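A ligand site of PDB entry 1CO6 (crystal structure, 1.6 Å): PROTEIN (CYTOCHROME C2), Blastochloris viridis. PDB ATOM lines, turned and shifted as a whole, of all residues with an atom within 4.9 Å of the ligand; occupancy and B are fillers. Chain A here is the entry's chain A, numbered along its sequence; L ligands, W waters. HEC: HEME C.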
ATOM      1  N   GLN A  12      12.365  19.029 -26.659  1.00  0.00           N
ATOM      2  CA  GLN A  12      12.944  18.540 -25.378  1.00  0.00           C
ATOM      3  C   GLN A  12      12.892  19.656 -24.361  1.00  0.00           C
ATOM      4  O   GLN A  12      12.440  19.473 -23.217  1.00  0.00           O
ATOM      5  CB  GLN A  12      14.277  17.861 -25.506  1.00  0.00           C
ATOM      6  CG  GLN A  12      15.232  18.093 -26.609  1.00  0.00           C
ATOM      7  CD  GLN A  12      16.395  17.128 -26.655  1.00  0.00           C
ATOM      8  OE1 GLN A  12      16.943  16.763 -27.728  1.00  0.00           O
ATOM      9  NE2 GLN A  12      16.892  16.683 -25.511  1.00  0.00           N
ATOM     10  N   CYS A  13      13.195  20.879 -24.763  1.00  0.00           N
ATOM     11  CA  CYS A  13      13.189  22.056 -23.910  1.00  0.00           C
ATOM     12  C   CYS A  13      11.796  22.542 -23.497  1.00  0.00           C
ATOM     13  O   CYS A  13      11.686  23.078 -22.394  1.00  0.00           O
ATOM     14  CB  CYS A  13      13.810  23.264 -24.680  1.00  0.00           C
ATOM     15  SG  CYS A  13      15.300  22.820 -25.626  1.00  0.00           S
ATOM     16  N   CYS A  16      10.050  22.295 -20.045  1.00  0.00           N
ATOM     17  CA  CYS A  16      10.381  23.239 -18.947  1.00  0.00           C
ATOM     18  C   CYS A  16      10.467  24.677 -19.321  1.00  0.00           C
ATOM     19  O   CYS A  16      10.409  25.522 -18.398  1.00  0.00           O
ATOM     20  CB  CYS A  16      11.682  22.780 -18.269  1.00  0.00           C
ATOM     21  SG  CYS A  16      11.754  21.038 -17.715  1.00  0.00           S
ATOM     22  N   HIS A  17      10.565  25.017 -20.589  1.00  0.00           N
ATOM     23  CA  HIS A  17      10.740  26.411 -21.011  1.00  0.00           C
ATOM     24  C   HIS A  17       9.723  26.818 -22.068  1.00  0.00           C
ATOM     25  O   HIS A  17       9.279  26.000 -22.898  1.00  0.00           O
ATOM     26  CB  HIS A  17      12.157  26.533 -21.665  1.00  0.00           C
ATOM     27  CG  HIS A  17      13.349  26.397 -20.790  1.00  0.00           C
ATOM     28  ND1 HIS A  17      13.785  27.407 -20.010  1.00  0.00           N
ATOM     29  CD2 HIS A  17      14.272  25.411 -20.706  1.00  0.00           C
ATOM     30  CE1 HIS A  17      14.881  26.985 -19.389  1.00  0.00           C
ATOM     31  NE2 HIS A  17      15.270  25.748 -19.796  1.00  0.00           N
ATOM     32  N   VAL A  27       9.050  25.592 -15.185  1.00  0.00           N
ATOM     33  CA  VAL A  27      10.087  24.992 -14.322  1.00  0.00           C
ATOM     34  C   VAL A  27      11.386  25.791 -14.658  1.00  0.00           C
ATOM     35  O   VAL A  27      12.176  26.023 -13.743  1.00  0.00           O
ATOM     36  CB  VAL A  27      10.262  23.475 -14.461  1.00  0.00           C
ATOM     37  CG1 VAL A  27      11.573  22.939 -13.863  1.00  0.00           C
ATOM     38  CG2 VAL A  27       9.110  22.738 -13.744  1.00  0.00           C
ATOM     39  N   GLY A  28      11.519  26.196 -15.919  1.00  0.00           N
ATOM     40  CA  GLY A  28      12.724  26.965 -16.321  1.00  0.00           C
ATOM     41  C   GLY A  28      12.235  28.329 -16.808  1.00  0.00           C
ATOM     42  O   GLY A  28      11.037  28.540 -17.078  1.00  0.00           O
ATOM     43  N   PRO A  29      13.166  29.244 -16.967  1.00  0.00           N
ATOM     44  CA  PRO A  29      12.836  30.617 -17.383  1.00  0.00           C
ATOM     45  C   PRO A  29      12.568  30.794 -18.865  1.00  0.00           C
ATOM     46  O   PRO A  29      13.038  29.959 -19.687  1.00  0.00           O
ATOM     47  CB  PRO A  29      14.068  31.448 -16.975  1.00  0.00           C
ATOM     48  CG  PRO A  29      15.234  30.482 -17.031  1.00  0.00           C
ATOM     49  CD  PRO A  29      14.621  29.101 -16.657  1.00  0.00           C
ATOM     50  N   LEU A  31      12.851  31.730 -22.669  1.00  0.00           N
ATOM     51  CA  LEU A  31      14.036  31.766 -23.532  1.00  0.00           C
ATOM     52  C   LEU A  31      13.943  32.781 -24.651  1.00  0.00           C
ATOM     53  O   LEU A  31      14.786  32.665 -25.559  1.00  0.00           O
ATOM     54  CB  LEU A  31      14.440  30.348 -24.001  1.00  0.00           C
ATOM     55  CG  LEU A  31      14.851  29.331 -22.963  1.00  0.00           C
ATOM     56  CD1 LEU A  31      15.199  28.005 -23.633  1.00  0.00           C
ATOM     57  CD2 LEU A  31      16.023  29.792 -22.068  1.00  0.00           C
ATOM     58  N   LEU A  34      17.327  35.192 -25.609  1.00  0.00           N
ATOM     59  CA  LEU A  34      18.400  34.549 -24.888  1.00  0.00           C
ATOM     60  C   LEU A  34      19.815  35.052 -25.239  1.00  0.00           C
ATOM     61  O   LEU A  34      20.587  35.370 -24.278  1.00  0.00           O
ATOM     62  CB  LEU A  34      18.287  33.007 -25.029  1.00  0.00           C
ATOM     63  CG  LEU A  34      19.470  32.301 -24.389  1.00  0.00           C
ATOM     64  CD1 LEU A  34      19.414  32.257 -22.848  1.00  0.00           C
ATOM     65  CD2 LEU A  34      19.504  30.871 -24.919  1.00  0.00           C
ATOM     66  N   ARG A  37      22.129  37.944 -23.462  1.00  0.00           N
ATOM     67  CA  ARG A  37      21.690  38.215 -22.055  1.00  0.00           C
ATOM     68  C   ARG A  37      22.631  37.576 -21.030  1.00  0.00           C
ATOM     69  O   ARG A  37      23.294  36.553 -21.311  1.00  0.00           O
ATOM     70  CB  ARG A  37      20.214  37.883 -21.958  1.00  0.00           C
ATOM     71  CG  ARG A  37      19.741  36.578 -21.350  1.00  0.00           C
ATOM     72  CD  ARG A  37      18.210  36.704 -21.158  1.00  0.00           C
ATOM     73  NE  ARG A  37      17.810  35.413 -20.590  1.00  0.00           N
ATOM     74  CZ  ARG A  37      16.775  34.623 -20.944  1.00  0.00           C
ATOM     75  NH1 ARG A  37      16.556  33.446 -20.316  1.00  0.00           N
ATOM     76  NH2 ARG A  37      15.940  34.959 -21.934  1.00  0.00           N
ATOM     77  N   HIS A  38      22.755  38.230 -19.877  1.00  0.00           N
ATOM     78  CA  HIS A  38      23.575  37.761 -18.727  1.00  0.00           C
ATOM     79  C   HIS A  38      22.763  36.674 -18.024  1.00  0.00           C
ATOM     80  O   HIS A  38      21.521  36.731 -17.939  1.00  0.00           O
ATOM     81  CB  HIS A  38      23.944  38.928 -17.768  1.00  0.00           C
ATOM     82  CG  HIS A  38      25.017  39.781 -18.384  1.00  0.00           C
ATOM     83  ND1 HIS A  38      26.275  39.962 -17.873  1.00  0.00           N
ATOM     84  CD2 HIS A  38      24.998  40.472 -19.563  1.00  0.00           C
ATOM     85  CE1 HIS A  38      26.965  40.754 -18.700  1.00  0.00           C
ATOM     86  NE2 HIS A  38      26.227  41.067 -19.738  1.00  0.00           N
ATOM     87  N   SER A  39      23.428  35.658 -17.543  1.00  0.00           N
ATOM     88  CA  SER A  39      22.673  34.559 -16.869  1.00  0.00           C
ATOM     89  C   SER A  39      22.006  35.075 -15.605  1.00  0.00           C
ATOM     90  O   SER A  39      22.498  36.023 -14.959  1.00  0.00           O
ATOM     91  CB  SER A  39      23.555  33.349 -16.563  1.00  0.00           C
ATOM     92  OG  SER A  39      24.611  33.700 -15.695  1.00  0.00           O
ATOM     93  N   GLY A  40      20.935  34.415 -15.234  1.00  0.00           N
ATOM     94  CA  GLY A  40      20.189  34.717 -14.026  1.00  0.00           C
ATOM     95  C   GLY A  40      19.476  36.038 -13.995  1.00  0.00           C
ATOM     96  O   GLY A  40      19.294  36.560 -12.852  1.00  0.00           O
ATOM     97  N   THR A  41      19.031  36.586 -15.114  1.00  0.00           N
ATOM     98  CA  THR A  41      18.362  37.877 -15.049  1.00  0.00           C
ATOM     99  C   THR A  41      16.906  37.898 -15.413  1.00  0.00           C
ATOM    100  O   THR A  41      16.400  39.039 -15.283  1.00  0.00           O
ATOM    101  CB  THR A  41      19.245  38.939 -15.816  1.00  0.00           C
ATOM    102  OG1 THR A  41      19.197  38.714 -17.245  1.00  0.00           O
ATOM    103  CG2 THR A  41      20.722  38.934 -15.337  1.00  0.00           C
ATOM    104  N   ILE A  42      16.212  36.857 -15.796  1.00  0.00           N
ATOM    105  CA  ILE A  42      14.766  36.936 -16.105  1.00  0.00           C
ATOM    106  C   ILE A  42      14.062  37.233 -14.785  1.00  0.00           C
ATOM    107  O   ILE A  42      14.285  36.532 -13.801  1.00  0.00           O
ATOM    108  CB  ILE A  42      14.158  35.669 -16.798  1.00  0.00           C
ATOM    109  CG1 ILE A  42      14.676  35.548 -18.254  1.00  0.00           C
ATOM    110  CG2 ILE A  42      12.574  35.615 -16.764  1.00  0.00           C
ATOM    111  CD1 ILE A  42      14.685  36.858 -19.108  1.00  0.00           C
ATOM    112  N   PHE A  45      12.034  34.761 -11.951  1.00  0.00           N
ATOM    113  CA  PHE A  45      12.464  33.354 -12.005  1.00  0.00           C
ATOM    114  C   PHE A  45      13.383  33.164 -10.794  1.00  0.00           C
ATOM    115  O   PHE A  45      14.216  34.033 -10.595  1.00  0.00           O
ATOM    116  CB  PHE A  45      13.131  32.909 -13.310  1.00  0.00           C
ATOM    117  CG  PHE A  45      13.396  31.393 -13.246  1.00  0.00           C
ATOM    118  CD1 PHE A  45      12.286  30.529 -13.429  1.00  0.00           C
ATOM    119  CD2 PHE A  45      14.647  30.887 -12.932  1.00  0.00           C
ATOM    120  CE1 PHE A  45      12.421  29.168 -13.342  1.00  0.00           C
ATOM    121  CE2 PHE A  45      14.829  29.521 -12.825  1.00  0.00           C
ATOM    122  CZ  PHE A  45      13.696  28.653 -13.043  1.00  0.00           C
ATOM    123  N   ALA A  46      13.184  32.062 -10.091  1.00  0.00           N
ATOM    124  CA  ALA A  46      14.014  31.723  -8.927  1.00  0.00           C
ATOM    125  C   ALA A  46      15.195  30.857  -9.367  1.00  0.00           C
ATOM    126  O   ALA A  46      15.244  29.626  -9.327  1.00  0.00           O
ATOM    127  CB  ALA A  46      13.177  31.051  -7.838  1.00  0.00           C
ATOM    128  N   TYR A  47      16.249  31.563  -9.727  1.00  0.00           N
ATOM    129  CA  TYR A  47      17.500  30.923 -10.176  1.00  0.00           C
ATOM    130  C   TYR A  47      18.304  30.371  -9.007  1.00  0.00           C
ATOM    131  O   TYR A  47      18.167  30.904  -7.877  1.00  0.00           O
ATOM    132  CB  TYR A  47      18.402  31.976 -10.856  1.00  0.00           C
ATOM    133  CG  TYR A  47      17.964  32.444 -12.230  1.00  0.00           C
ATOM    134  CD1 TYR A  47      17.268  33.631 -12.381  1.00  0.00           C
ATOM    135  CD2 TYR A  47      18.290  31.681 -13.349  1.00  0.00           C
ATOM    136  CE1 TYR A  47      16.866  34.072 -13.640  1.00  0.00           C
ATOM    137  CE2 TYR A  47      17.922  32.118 -14.631  1.00  0.00           C
ATOM    138  CZ  TYR A  47      17.215  33.301 -14.764  1.00  0.00           C
ATOM    139  OH  TYR A  47      16.889  33.750 -16.009  1.00  0.00           O
ATOM    140  N   SER A  48      19.082  29.363  -9.329  1.00  0.00           N
ATOM    141  CA  SER A  48      20.008  28.797  -8.339  1.00  0.00           C
ATOM    142  C   SER A  48      21.147  29.846  -8.209  1.00  0.00           C
ATOM    143  O   SER A  48      21.331  30.716  -9.076  1.00  0.00           O
ATOM    144  CB  SER A  48      20.700  27.526  -8.753  1.00  0.00           C
ATOM    145  OG  SER A  48      21.381  27.713  -9.996  1.00  0.00           O
ATOM    146  N   ASN A  51      23.613  29.383 -11.082  1.00  0.00           N
ATOM    147  CA  ASN A  51      23.427  30.116 -12.331  1.00  0.00           C
ATOM    148  C   ASN A  51      23.569  31.628 -12.149  1.00  0.00           C
ATOM    149  O   ASN A  51      24.355  32.317 -12.838  1.00  0.00           O
ATOM    150  CB  ASN A  51      22.047  29.705 -12.904  1.00  0.00           C
ATOM    151  CG  ASN A  51      21.690  30.577 -14.095  1.00  0.00           C
ATOM    152  OD1 ASN A  51      21.516  31.813 -13.975  1.00  0.00           O
ATOM    153  ND2 ASN A  51      21.606  29.997 -15.272  1.00  0.00           N
ATOM    154  N   TRP A  58      25.347  34.878 -22.270  1.00  0.00           N
ATOM    155  CA  TRP A  58      24.975  33.857 -23.262  1.00  0.00           C
ATOM    156  C   TRP A  58      25.253  34.211 -24.713  1.00  0.00           C
ATOM    157  O   TRP A  58      24.413  34.777 -25.398  1.00  0.00           O
ATOM    158  CB  TRP A  58      23.488  33.462 -23.106  1.00  0.00           C
ATOM    159  CG  TRP A  58      23.206  32.823 -21.799  1.00  0.00           C
ATOM    160  CD1 TRP A  58      22.473  33.346 -20.786  1.00  0.00           C
ATOM    161  CD2 TRP A  58      23.658  31.539 -21.351  1.00  0.00           C
ATOM    162  NE1 TRP A  58      22.414  32.443 -19.745  1.00  0.00           N
ATOM    163  CE2 TRP A  58      23.103  31.327 -20.080  1.00  0.00           C
ATOM    164  CE3 TRP A  58      24.439  30.527 -21.941  1.00  0.00           C
ATOM    165  CZ2 TRP A  58      23.378  30.176 -19.327  1.00  0.00           C
ATOM    166  CZ3 TRP A  58      24.697  29.381 -21.212  1.00  0.00           C
ATOM    167  CH2 TRP A  58      24.149  29.189 -19.942  1.00  0.00           C
ATOM    168  N   PHE A  63      26.730  29.047 -25.231  1.00  0.00           N
ATOM    169  CA  PHE A  63      25.496  28.213 -25.227  1.00  0.00           C
ATOM    170  C   PHE A  63      25.833  26.789 -25.688  1.00  0.00           C
ATOM    171  O   PHE A  63      25.381  25.763 -25.170  1.00  0.00           O
ATOM    172  CB  PHE A  63      24.391  28.837 -26.076  1.00  0.00           C
ATOM    173  CG  PHE A  63      23.156  27.999 -26.288  1.00  0.00           C
ATOM    174  CD1 PHE A  63      22.154  28.030 -25.296  1.00  0.00           C
ATOM    175  CD2 PHE A  63      22.985  27.207 -27.408  1.00  0.00           C
ATOM    176  CE1 PHE A  63      20.960  27.291 -25.463  1.00  0.00           C
ATOM    177  CE2 PHE A  63      21.841  26.404 -27.567  1.00  0.00           C
ATOM    178  CZ  PHE A  63      20.820  26.482 -26.596  1.00  0.00           C
ATOM    179  N   TYR A  66      27.619  24.844 -22.980  1.00  0.00           N
ATOM    180  CA  TYR A  66      26.690  24.558 -21.895  1.00  0.00           C
ATOM    181  C   TYR A  66      25.719  23.467 -22.254  1.00  0.00           C
ATOM    182  O   TYR A  66      25.497  22.513 -21.516  1.00  0.00           O
ATOM    183  CB  TYR A  66      25.887  25.828 -21.545  1.00  0.00           C
ATOM    184  CG  TYR A  66      24.726  25.681 -20.609  1.00  0.00           C
ATOM    185  CD1 TYR A  66      23.407  25.670 -21.086  1.00  0.00           C
ATOM    186  CD2 TYR A  66      24.947  25.526 -19.223  1.00  0.00           C
ATOM    187  CE1 TYR A  66      22.318  25.554 -20.223  1.00  0.00           C
ATOM    188  CE2 TYR A  66      23.852  25.414 -18.331  1.00  0.00           C
ATOM    189  CZ  TYR A  66      22.564  25.403 -18.853  1.00  0.00           C
ATOM    190  OH  TYR A  66      21.525  25.321 -17.996  1.00  0.00           O
ATOM    191  N   ILE A  67      25.077  23.605 -23.402  1.00  0.00           N
ATOM    192  CA  ILE A  67      24.056  22.636 -23.809  1.00  0.00           C
ATOM    193  C   ILE A  67      24.565  21.213 -24.009  1.00  0.00           C
ATOM    194  O   ILE A  67      23.735  20.278 -23.776  1.00  0.00           O
ATOM    195  CB  ILE A  67      23.178  23.260 -24.932  1.00  0.00           C
ATOM    196  CG1 ILE A  67      21.694  22.893 -24.832  1.00  0.00           C
ATOM    197  CG2 ILE A  67      23.822  22.855 -26.310  1.00  0.00           C
ATOM    198  CD1 ILE A  67      20.941  23.253 -23.520  1.00  0.00           C
ATOM    199  N   THR A  77      23.649  23.463 -10.989  1.00  0.00           N
ATOM    200  CA  THR A  77      22.461  24.076 -11.636  1.00  0.00           C
ATOM    201  C   THR A  77      21.203  23.240 -11.399  1.00  0.00           C
ATOM    202  O   THR A  77      21.275  21.998 -11.332  1.00  0.00           O
ATOM    203  CB  THR A  77      22.702  24.316 -13.180  1.00  0.00           C
ATOM    204  OG1 THR A  77      21.488  24.974 -13.623  1.00  0.00           O
ATOM    205  CG2 THR A  77      22.929  23.077 -14.051  1.00  0.00           C
ATOM    206  N   LYS A  78      20.084  23.863 -11.292  1.00  0.00           N
ATOM    207  CA  LYS A  78      18.765  23.246 -11.131  1.00  0.00           C
ATOM    208  C   LYS A  78      18.300  22.571 -12.452  1.00  0.00           C
ATOM    209  O   LYS A  78      17.289  21.841 -12.491  1.00  0.00           O
ATOM    210  CB  LYS A  78      17.706  24.245 -10.698  1.00  0.00           C
ATOM    211  CG  LYS A  78      17.645  25.006  -9.423  1.00  0.00           C
ATOM    212  CD  LYS A  78      16.410  25.931  -9.416  1.00  0.00           C
ATOM    213  CE  LYS A  78      16.582  27.021  -8.360  1.00  0.00           C
ATOM    214  NZ  LYS A  78      15.363  27.697  -7.859  1.00  0.00           N
ATOM    215  N   MET A  79      18.983  22.819 -13.569  1.00  0.00           N
ATOM    216  CA  MET A  79      18.695  22.263 -14.883  1.00  0.00           C
ATOM    217  C   MET A  79      19.285  20.883 -14.981  1.00  0.00           C
ATOM    218  O   MET A  79      20.408  20.684 -15.511  1.00  0.00           O
ATOM    219  CB  MET A  79      19.109  23.202 -16.044  1.00  0.00           C
ATOM    220  CG  MET A  79      18.717  22.553 -17.374  1.00  0.00           C
ATOM    221  SD  MET A  79      18.896  23.802 -18.722  1.00  0.00           S
ATOM    222  CE  MET A  79      19.397  22.635 -20.003  1.00  0.00           C
ATOM    223  N   ILE A  80      18.532  19.874 -14.474  1.00  0.00           N
ATOM    224  CA  ILE A  80      18.991  18.465 -14.490  1.00  0.00           C
ATOM    225  C   ILE A  80      18.511  17.875 -15.816  1.00  0.00           C
ATOM    226  O   ILE A  80      17.359  17.486 -15.976  1.00  0.00           O
ATOM    227  CB  ILE A  80      18.574  17.665 -13.216  1.00  0.00           C
ATOM    228  CG1 ILE A  80      19.094  18.413 -11.927  1.00  0.00           C
ATOM    229  CG2 ILE A  80      19.094  16.211 -13.286  1.00  0.00           C
ATOM    230  CD1 ILE A  80      18.075  18.212 -10.718  1.00  0.00           C
ATOM    231  N   PHE A  81      19.451  17.874 -16.753  1.00  0.00           N
ATOM    232  CA  PHE A  81      19.201  17.497 -18.168  1.00  0.00           C
ATOM    233  C   PHE A  81      20.507  16.992 -18.719  1.00  0.00           C
ATOM    234  O   PHE A  81      21.524  17.662 -18.453  1.00  0.00           O
ATOM    235  CB  PHE A  81      18.670  18.784 -18.837  1.00  0.00           C
ATOM    236  CG  PHE A  81      18.522  18.759 -20.326  1.00  0.00           C
ATOM    237  CD1 PHE A  81      17.414  18.064 -20.864  1.00  0.00           C
ATOM    238  CD2 PHE A  81      19.454  19.327 -21.195  1.00  0.00           C
ATOM    239  CE1 PHE A  81      17.247  17.998 -22.248  1.00  0.00           C
ATOM    240  CE2 PHE A  81      19.280  19.253 -22.579  1.00  0.00           C
ATOM    241  CZ  PHE A  81      18.168  18.575 -23.100  1.00  0.00           C
ATOM    242  N   VAL A  84      22.544  18.109 -25.016  1.00  0.00           N
ATOM    243  CA  VAL A  84      22.358  17.782 -26.467  1.00  0.00           C
ATOM    244  C   VAL A  84      23.797  17.622 -26.992  1.00  0.00           C
ATOM    245  O   VAL A  84      24.577  18.557 -27.081  1.00  0.00           O
ATOM    246  CB  VAL A  84      21.438  18.738 -27.185  1.00  0.00           C
ATOM    247  CG1 VAL A  84      21.181  18.371 -28.675  1.00  0.00           C
ATOM    248  CG2 VAL A  84      20.072  18.975 -26.523  1.00  0.00           C
ATOM    249  N   LEU A  93      19.123  24.072 -33.176  1.00  0.00           N
ATOM    250  CA  LEU A  93      18.531  24.672 -31.972  1.00  0.00           C
ATOM    251  C   LEU A  93      18.814  26.159 -31.850  1.00  0.00           C
ATOM    252  O   LEU A  93      17.922  26.970 -31.521  1.00  0.00           O
ATOM    253  CB  LEU A  93      19.126  23.820 -30.819  1.00  0.00           C
ATOM    254  CG  LEU A  93      18.674  24.330 -29.439  1.00  0.00           C
ATOM    255  CD1 LEU A  93      17.162  24.189 -29.358  1.00  0.00           C
ATOM    256  CD2 LEU A  93      19.423  23.513 -28.374  1.00  0.00           C
ATOM    257  N   ILE A  97      16.073  29.354 -31.700  1.00  0.00           N
ATOM    258  CA  ILE A  97      15.998  30.291 -30.588  1.00  0.00           C
ATOM    259  C   ILE A  97      16.294  31.721 -31.043  1.00  0.00           C
ATOM    260  O   ILE A  97      15.662  32.645 -30.504  1.00  0.00           O
ATOM    261  CB  ILE A  97      16.896  29.828 -29.392  1.00  0.00           C
ATOM    262  CG1 ILE A  97      16.380  28.468 -28.816  1.00  0.00           C
ATOM    263  CG2 ILE A  97      16.959  30.909 -28.264  1.00  0.00           C
ATOM    264  CD1 ILE A  97      17.380  27.922 -27.732  1.00  0.00           C
HETATM  265 FE   HEC L   1      16.917  24.732 -19.368  1.00  0.00          FE
HETATM  266  CHA HEC L   1      17.980  27.207 -17.385  1.00  0.00           C
HETATM  267  CHB HEC L   1      18.299  26.277 -22.098  1.00  0.00           C
HETATM  268  CHC HEC L   1      16.036  22.038 -21.374  1.00  0.00           C
HETATM  269  CHD HEC L   1      15.115  23.369 -16.749  1.00  0.00           C
HETATM  270  NA  HEC L   1      17.933  26.445 -19.692  1.00  0.00           N
HETATM  271  C1A HEC L   1      18.417  27.299 -18.704  1.00  0.00           C
HETATM  272  C2A HEC L   1      19.306  28.250 -19.309  1.00  0.00           C
HETATM  273  C3A HEC L   1      19.392  27.970 -20.610  1.00  0.00           C
HETATM  274  C4A HEC L   1      18.549  26.832 -20.885  1.00  0.00           C
HETATM  275  CMA HEC L   1      20.229  28.685 -21.706  1.00  0.00           C
HETATM  276  CAA HEC L   1      19.953  29.460 -18.559  1.00  0.00           C
HETATM  277  CBA HEC L   1      18.904  30.608 -18.527  1.00  0.00           C
HETATM  278  CGA HEC L   1      19.310  31.923 -17.913  1.00  0.00           C
HETATM  279  O1A HEC L   1      20.456  32.025 -17.515  1.00  0.00           O
HETATM  280  O2A HEC L   1      18.395  32.784 -17.873  1.00  0.00           O
HETATM  281  NB  HEC L   1      17.097  24.264 -21.313  1.00  0.00           N
HETATM  282  C1B HEC L   1      17.658  25.091 -22.294  1.00  0.00           C
HETATM  283  C2B HEC L   1      17.557  24.405 -23.561  1.00  0.00           C
HETATM  284  C3B HEC L   1      16.972  23.229 -23.346  1.00  0.00           C
HETATM  285  C4B HEC L   1      16.645  23.123 -21.963  1.00  0.00           C
HETATM  286  CMB HEC L   1      18.078  25.034 -24.872  1.00  0.00           C
HETATM  287  CAB HEC L   1      16.632  22.182 -24.462  1.00  0.00           C
HETATM  288  CBB HEC L   1      17.749  21.496 -24.993  1.00  0.00           C
HETATM  289  NC  HEC L   1      15.804  23.049 -19.099  1.00  0.00           N
HETATM  290  C1C HEC L   1      15.588  22.068 -20.046  1.00  0.00           C
HETATM  291  C2C HEC L   1      14.758  21.046 -19.438  1.00  0.00           C
HETATM  292  C3C HEC L   1      14.531  21.380 -18.163  1.00  0.00           C
HETATM  293  C4C HEC L   1      15.157  22.665 -17.933  1.00  0.00           C
HETATM  294  CMC HEC L   1      14.296  19.764 -20.172  1.00  0.00           C
HETATM  295  CAC HEC L   1      13.622  20.600 -17.134  1.00  0.00           C
HETATM  296  CBC HEC L   1      13.885  19.257 -16.818  1.00  0.00           C
HETATM  297  ND  HEC L   1      16.579  25.233 -17.460  1.00  0.00           N
HETATM  298  C1D HEC L   1      15.849  24.504 -16.506  1.00  0.00           C
HETATM  299  C2D HEC L   1      16.023  25.158 -15.209  1.00  0.00           C
HETATM  300  C3D HEC L   1      16.796  26.231 -15.382  1.00  0.00           C
HETATM  301  C4D HEC L   1      17.170  26.277 -16.778  1.00  0.00           C
HETATM  302  CMD HEC L   1      15.367  24.622 -13.909  1.00  0.00           C
HETATM  303  CAD HEC L   1      17.334  27.212 -14.310  1.00  0.00           C
HETATM  304  CBD HEC L   1      18.768  26.787 -13.868  1.00  0.00           C
HETATM  305  CGD HEC L   1      19.179  27.332 -12.519  1.00  0.00           C
HETATM  306  O1D HEC L   1      20.207  26.718 -12.088  1.00  0.00           O
HETATM  307  O2D HEC L   1      18.565  28.279 -11.969  1.00  0.00           O
HETATM  308  O   HOH W   1      21.659  26.996 -15.696  1.00  0.00           O
HETATM  309  O   HOH W   2      16.087  20.751 -14.648  1.00  0.00           O
HETATM  310  O   HOH W   3      19.185  35.482 -17.978  1.00  0.00           O
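The backbone carbonyl oxygen (O) of Cys 16 sits at hydrogen-bond distance from the backbone NH (N) of Val 27. N of Gly 28 lies within hydrogen-bond range of O of Cys 16 (2.8 Å). The backbone NH (N) of Met 79 sits close to the side-chain hydroxyl (OG1) of Thr 77 (3.3 Å). SD of Met 79 sits close to OH of Tyr 66. The side-chain hydroxyl of Tyr 47 is in hydrogen-bond range of the backbone NH of Ile 42. OG of Ser 48 sits at hydrogen-bond distance from N of Asn 51, 3.0 Å away. The backbone NH of Trp 58 is in hydrogen-bond range of the backbone carbonyl oxygen of Arg 37 (2.8 Å). N of Val 84 lies within hydrogen-bond range of O of Ile 67 (2.8 Å).
Residues that only touch the ligand: Gln 12 (3.6 Å), Val 27 (3.5 Å), Gly 28 (3.9 Å), Pro 29 (3.8 Å), Leu 31 (3.9 Å), Leu 34 (3.8 Å), Ser 39 (3.4 Å), Phe 45 (3.7 Å), Phe 63 (3.5 Å), Tyr 66 (3.8 Å), Ile 67 (3.6 Å), Ile 80 (3.99 Å), Phe 81 (3.5 Å) and Val 84 (3.8 Å). Hydrophobic or aromatic side chains within 4 Å of the ligand: His 17, Pro 29, Leu 31, Leu 34, Phe 45, Tyr 47, Trp 58, Phe 63, Tyr 66, Ile 67, Met 79, Phe 81 and Val 84. The nearest printed residue that does not touch the ligand is Leu 93 (4.05 Å).
Water W1 lies within hydrogen-bond range of OH of Tyr 66 (2.8 Å), OG1 of Thr 77 (2.9 Å) and ND2 of Asn 51 (3.0 Å).
A carbon (CAB) of the ligand is covalently linked to the side-chain sulfur (SG) of Cys 13, 1.9 Å away. NE2 of His 17 is bound to FE of the ligand (2.0 Å). A carbon (CAC) of the ligand is covalently linked to the side-chain sulfur (SG) of Cys 16, 2.0 Å away. The side-chain sulfur (SD) of Met 79 binds an iron atom (FE) of the ligand (2.3 Å). The side-chain hydroxyl (OH) of Tyr 47 lies within hydrogen-bond range of an oxygen (O2A) of the ligand, 2.6 Å away. The backbone NH (N) of Ser 48 sits at hydrogen-bond distance from an oxygen (O2D) of the ligand (2.9 Å). The side-chain hydroxyl (OG) of Ser 48 lies within hydrogen-bond range of an oxygen (O1D) of the ligand (2.6 Å). The side-chain hydroxyl (OG1) of Thr 77 lies within hydrogen-bond range of an oxygen (O1D) of the ligand (2.7 Å). The backbone NH (N) of Lys 78 lies within hydrogen-bond range of an oxygen (O1D) of the ligand (3.0 Å). An oxygen (O1A) of the ligand sits at hydrogen-bond distance from the indole nitrogen (NE1) of Trp 58 (3.0 Å). NH1 of Arg 37 lies within salt-bridge range of O2A of the ligand (3.1 Å). An oxygen (O1A) of the ligand sits at hydrogen-bond distance from the side-chain amide nitrogen of Asn 51. The backbone NH (N) of Gly 40 lies within hydrogen-bond range of an oxygen (O1A) of the ligand, at 3.3 Å.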
